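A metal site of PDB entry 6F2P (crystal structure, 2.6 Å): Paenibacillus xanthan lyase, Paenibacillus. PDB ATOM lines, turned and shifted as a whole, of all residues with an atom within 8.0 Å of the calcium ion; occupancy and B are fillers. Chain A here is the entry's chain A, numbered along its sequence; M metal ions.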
ATOM      1  N   TYR A 466      -0.949 -19.827  33.098  1.00  0.00           N
ATOM      2  CA  TYR A 466      -0.171 -20.846  32.416  1.00  0.00           C
ATOM      3  C   TYR A 466      -0.584 -22.210  32.946  1.00  0.00           C
ATOM      4  O   TYR A 466      -0.889 -22.354  34.126  1.00  0.00           O
ATOM      5  CB  TYR A 466       1.338 -20.589  32.598  1.00  0.00           C
ATOM      6  CG  TYR A 466       1.715 -19.149  32.367  1.00  0.00           C
ATOM      7  CD1 TYR A 466       1.334 -18.490  31.201  1.00  0.00           C
ATOM      8  CD2 TYR A 466       2.417 -18.414  33.331  1.00  0.00           C
ATOM      9  CE1 TYR A 466       1.649 -17.159  30.993  1.00  0.00           C
ATOM     10  CE2 TYR A 466       2.745 -17.073  33.119  1.00  0.00           C
ATOM     11  CZ  TYR A 466       2.357 -16.458  31.942  1.00  0.00           C
ATOM     12  OH  TYR A 466       2.664 -15.128  31.728  1.00  0.00           O
ATOM     13  N   PHE A 489       1.424 -21.737  27.390  1.00  0.00           N
ATOM     14  CA  PHE A 489       2.144 -20.612  27.983  1.00  0.00           C
ATOM     15  C   PHE A 489       1.573 -19.259  27.561  1.00  0.00           C
ATOM     16  O   PHE A 489       0.359 -19.111  27.480  1.00  0.00           O
ATOM     17  CB  PHE A 489       3.644 -20.694  27.695  1.00  0.00           C
ATOM     18  CG  PHE A 489       4.289 -21.962  28.215  1.00  0.00           C
ATOM     19  CD1 PHE A 489       4.370 -22.201  29.584  1.00  0.00           C
ATOM     20  CD2 PHE A 489       4.801 -22.914  27.346  1.00  0.00           C
ATOM     21  CE1 PHE A 489       4.970 -23.365  30.071  1.00  0.00           C
ATOM     22  CE2 PHE A 489       5.385 -24.071  27.818  1.00  0.00           C
ATOM     23  CZ  PHE A 489       5.474 -24.299  29.192  1.00  0.00           C
ATOM     24  N   ASP A 490       2.430 -18.273  27.328  1.00  0.00           N
ATOM     25  CA  ASP A 490       1.911 -16.949  27.009  1.00  0.00           C
ATOM     26  C   ASP A 490       1.453 -16.784  25.560  1.00  0.00           C
ATOM     27  O   ASP A 490       0.467 -16.118  25.300  1.00  0.00           O
ATOM     28  CB  ASP A 490       2.903 -15.834  27.397  1.00  0.00           C
ATOM     29  CG  ASP A 490       4.267 -16.029  26.791  1.00  0.00           C
ATOM     30  OD1 ASP A 490       4.596 -17.187  26.486  1.00  0.00           O
ATOM     31  OD2 ASP A 490       5.017 -15.040  26.625  1.00  0.00           O
ATOM     32  N   ASP A 491       2.159 -17.411  24.616  1.00  0.00           N
ATOM     33  CA  ASP A 491       1.825 -17.256  23.209  1.00  0.00           C
ATOM     34  C   ASP A 491       2.137 -18.511  22.419  1.00  0.00           C
ATOM     35  O   ASP A 491       2.224 -18.482  21.197  1.00  0.00           O
ATOM     36  CB  ASP A 491       2.534 -16.050  22.592  1.00  0.00           C
ATOM     37  CG  ASP A 491       4.065 -16.133  22.716  1.00  0.00           C
ATOM     38  OD1 ASP A 491       4.570 -17.098  23.320  1.00  0.00           O
ATOM     39  OD2 ASP A 491       4.743 -15.204  22.236  1.00  0.00           O
ATOM     40  N   GLU A 492       2.337 -19.625  23.113  1.00  0.00           N
ATOM     41  CA  GLU A 492       2.545 -20.897  22.438  1.00  0.00           C
ATOM     42  C   GLU A 492       1.863 -22.021  23.194  1.00  0.00           C
ATOM     43  O   GLU A 492       1.641 -21.920  24.407  1.00  0.00           O
ATOM     44  CB  GLU A 492       4.044 -21.221  22.306  1.00  0.00           C
ATOM     45  CG  GLU A 492       4.774 -21.402  23.617  1.00  0.00           C
ATOM     46  CD  GLU A 492       5.395 -20.112  24.131  1.00  0.00           C
ATOM     47  OE1 GLU A 492       4.724 -19.409  24.902  1.00  0.00           O
ATOM     48  OE2 GLU A 492       6.555 -19.799  23.751  1.00  0.00           O
ATOM     49  N   ILE A 493       1.543 -23.088  22.464  1.00  0.00           N
ATOM     50  CA  ILE A 493       1.115 -24.334  23.064  1.00  0.00           C
ATOM     51  C   ILE A 493       2.049 -25.454  22.616  1.00  0.00           C
ATOM     52  O   ILE A 493       2.229 -25.655  21.415  1.00  0.00           O
ATOM     53  CB  ILE A 493      -0.314 -24.719  22.671  1.00  0.00           C
ATOM     54  CG1 ILE A 493      -1.302 -23.665  23.154  1.00  0.00           C
ATOM     55  CG2 ILE A 493      -0.667 -26.074  23.237  1.00  0.00           C
ATOM     56  CD1 ILE A 493      -1.973 -22.914  22.053  1.00  0.00           C
ATOM     57  N   LEU A 620       1.795 -22.007  17.321  1.00  0.00           N
ATOM     58  CA  LEU A 620       2.186 -20.610  17.404  1.00  0.00           C
ATOM     59  C   LEU A 620       1.130 -19.737  16.748  1.00  0.00           C
ATOM     60  O   LEU A 620       1.290 -19.322  15.601  1.00  0.00           O
ATOM     61  CB  LEU A 620       3.538 -20.404  16.717  1.00  0.00           C
ATOM     62  CG  LEU A 620       4.712 -21.172  17.331  1.00  0.00           C
ATOM     63  CD1 LEU A 620       5.953 -21.090  16.457  1.00  0.00           C
ATOM     64  CD2 LEU A 620       5.035 -20.662  18.737  1.00  0.00           C
ATOM     65  N   LYS A 623       0.886 -15.441  14.463  1.00  0.00           N
ATOM     66  CA  LYS A 623       2.227 -14.976  14.113  1.00  0.00           C
ATOM     67  C   LYS A 623       2.423 -14.946  12.611  1.00  0.00           C
ATOM     68  O   LYS A 623       1.891 -15.791  11.881  1.00  0.00           O
ATOM     69  CB  LYS A 623       3.304 -15.851  14.760  1.00  0.00           C
ATOM     70  CG  LYS A 623       3.783 -15.346  16.087  1.00  0.00           C
ATOM     71  CD  LYS A 623       4.762 -16.322  16.752  1.00  0.00           C
ATOM     72  CE  LYS A 623       5.269 -15.755  18.077  1.00  0.00           C
ATOM     73  NZ  LYS A 623       4.173 -15.012  18.784  1.00  0.00           N
ATOM     74  N   TYR A 631      10.883 -17.967  15.605  1.00  0.00           N
ATOM     75  CA  TYR A 631      10.687 -18.809  16.770  1.00  0.00           C
ATOM     76  C   TYR A 631      11.424 -20.137  16.597  1.00  0.00           C
ATOM     77  O   TYR A 631      12.053 -20.629  17.528  1.00  0.00           O
ATOM     78  CB  TYR A 631       9.188 -19.066  17.010  1.00  0.00           C
ATOM     79  CG  TYR A 631       8.831 -19.677  18.349  1.00  0.00           C
ATOM     80  CD1 TYR A 631       8.966 -21.048  18.576  1.00  0.00           C
ATOM     81  CD2 TYR A 631       8.304 -18.905  19.376  1.00  0.00           C
ATOM     82  CE1 TYR A 631       8.620 -21.614  19.795  1.00  0.00           C
ATOM     83  CE2 TYR A 631       7.952 -19.460  20.601  1.00  0.00           C
ATOM     84  CZ  TYR A 631       8.113 -20.815  20.807  1.00  0.00           C
ATOM     85  OH  TYR A 631       7.760 -21.369  22.031  1.00  0.00           O
ATOM     86  N   PRO A 635      13.858 -21.068  19.822  1.00  0.00           N
ATOM     87  CA  PRO A 635      12.597 -21.390  20.491  1.00  0.00           C
ATOM     88  C   PRO A 635      12.573 -20.874  21.905  1.00  0.00           C
ATOM     89  O   PRO A 635      13.586 -20.964  22.588  1.00  0.00           O
ATOM     90  CB  PRO A 635      12.591 -22.922  20.511  1.00  0.00           C
ATOM     91  CG  PRO A 635      13.551 -23.334  19.460  1.00  0.00           C
ATOM     92  CD  PRO A 635      14.605 -22.280  19.433  1.00  0.00           C
ATOM     93  N   GLN A 636      11.435 -20.347  22.330  1.00  0.00           N
ATOM     94  CA  GLN A 636      11.264 -19.884  23.697  1.00  0.00           C
ATOM     95  C   GLN A 636      10.888 -21.049  24.616  1.00  0.00           C
ATOM     96  O   GLN A 636      10.628 -20.832  25.800  1.00  0.00           O
ATOM     97  CB  GLN A 636      10.205 -18.786  23.777  1.00  0.00           C
ATOM     98  CG  GLN A 636      10.319 -17.710  22.706  1.00  0.00           C
ATOM     99  CD  GLN A 636       9.075 -16.850  22.652  1.00  0.00           C
ATOM    100  OE1 GLN A 636       8.160 -17.015  23.449  1.00  0.00           O
ATOM    101  NE2 GLN A 636       9.021 -15.934  21.697  1.00  0.00           N
ATOM    102  N   ILE A 637      10.854 -22.273  24.084  1.00  0.00           N
ATOM    103  CA  ILE A 637      10.583 -23.457  24.910  1.00  0.00           C
ATOM    104  C   ILE A 637      11.697 -24.499  24.799  1.00  0.00           C
ATOM    105  O   ILE A 637      12.384 -24.580  23.779  1.00  0.00           O
ATOM    106  CB  ILE A 637       9.228 -24.125  24.573  1.00  0.00           C
ATOM    107  CG1 ILE A 637       9.213 -24.600  23.116  1.00  0.00           C
ATOM    108  CG2 ILE A 637       8.059 -23.179  24.857  1.00  0.00           C
ATOM    109  CD1 ILE A 637       9.397 -26.087  22.957  1.00  0.00           C
ATOM    110  N   GLU A 651       9.320 -23.006  29.407  1.00  0.00           N
ATOM    111  CA  GLU A 651       9.339 -21.788  28.611  1.00  0.00           C
ATOM    112  C   GLU A 651      10.401 -20.890  29.223  1.00  0.00           C
ATOM    113  O   GLU A 651      10.235 -20.410  30.339  1.00  0.00           O
ATOM    114  CB  GLU A 651       7.969 -21.102  28.658  1.00  0.00           C
ATOM    115  CG  GLU A 651       7.603 -20.330  27.401  1.00  0.00           C
ATOM    116  CD  GLU A 651       8.107 -18.889  27.398  1.00  0.00           C
ATOM    117  OE1 GLU A 651       7.829 -18.179  26.415  1.00  0.00           O
ATOM    118  OE2 GLU A 651       8.781 -18.469  28.377  1.00  0.00           O
ATOM    119  N   THR A 652      11.492 -20.677  28.485  1.00  0.00           N
ATOM    120  CA  THR A 652      12.684 -20.040  29.063  1.00  0.00           C
ATOM    121  C   THR A 652      12.600 -18.522  29.221  1.00  0.00           C
ATOM    122  O   THR A 652      13.431 -17.920  29.897  1.00  0.00           O
ATOM    123  CB  THR A 652      13.944 -20.382  28.266  1.00  0.00           C
ATOM    124  OG1 THR A 652      13.810 -19.912  26.923  1.00  0.00           O
ATOM    125  CG2 THR A 652      14.171 -21.894  28.268  1.00  0.00           C
ATOM    126  N   GLN A 653      11.602 -17.905  28.602  1.00  0.00           N
ATOM    127  CA  GLN A 653      11.372 -16.482  28.801  1.00  0.00           C
ATOM    128  C   GLN A 653      10.641 -16.284  30.120  1.00  0.00           C
ATOM    129  O   GLN A 653      11.010 -15.426  30.920  1.00  0.00           O
ATOM    130  CB  GLN A 653      10.505 -15.904  27.677  1.00  0.00           C
ATOM    131  CG  GLN A 653      11.067 -16.108  26.296  1.00  0.00           C
ATOM    132  CD  GLN A 653      11.904 -14.927  25.832  1.00  0.00           C
ATOM    133  OE1 GLN A 653      11.506 -14.188  24.941  1.00  0.00           O
ATOM    134  NE2 GLN A 653      13.083 -14.752  26.455  1.00  0.00           N
ATOM    135  N   LEU A 654       9.590 -17.075  30.320  1.00  0.00           N
ATOM    136  CA  LEU A 654       8.748 -16.949  31.504  1.00  0.00           C
ATOM    137  C   LEU A 654       9.374 -17.633  32.725  1.00  0.00           C
ATOM    138  O   LEU A 654       8.961 -17.398  33.868  1.00  0.00           O
ATOM    139  CB  LEU A 654       7.385 -17.593  31.235  1.00  0.00           C
ATOM    140  CG  LEU A 654       6.476 -16.945  30.193  1.00  0.00           C
ATOM    141  CD1 LEU A 654       5.233 -17.795  30.002  1.00  0.00           C
ATOM    142  CD2 LEU A 654       6.106 -15.549  30.652  1.00  0.00           C
HETATM  143 CA    CA M   1       6.408 -17.528  24.816  1.00  0.00          CA
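Of the 16 residues printed, 5 come within 4 Å of the calcium ion.
The nearest printed residue that does not touch the calcium ion is Tyr 631 (4.9 Å).
The calcium ion is bound by OE1 of Glu 651 (2.2 Å), OE1 of Gln 636 (2.3 Å), OD1 of Asp 491 (2.4 Å), OD1 of Asp 490 (2.5 Å), OE2 of Glu 492 (2.5 Å) and OE1 of Glu 492 (2.5 Å).
The calcium ion has six donor atoms within binding distance.
OE2 of Glu 651 lies within hydrogen-bond range of N of Gln 653, at 2.9 Å.
The side-chain carboxylate (OE2) of Glu 651 is in hydrogen-bond range of the backbone NH (N) of Leu 654 (2.5 Å).
The backbone carbonyl oxygen of Gln 636 sits at hydrogen-bond distance from the backbone NH of Thr 652 (2.8 Å).
OD2 of Asp 491 is in salt-bridge range of NZ of Lys 623 (3.5 Å).
The side-chain carboxylate of Glu 492 sits close to the side-chain hydroxyl of Tyr 631.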
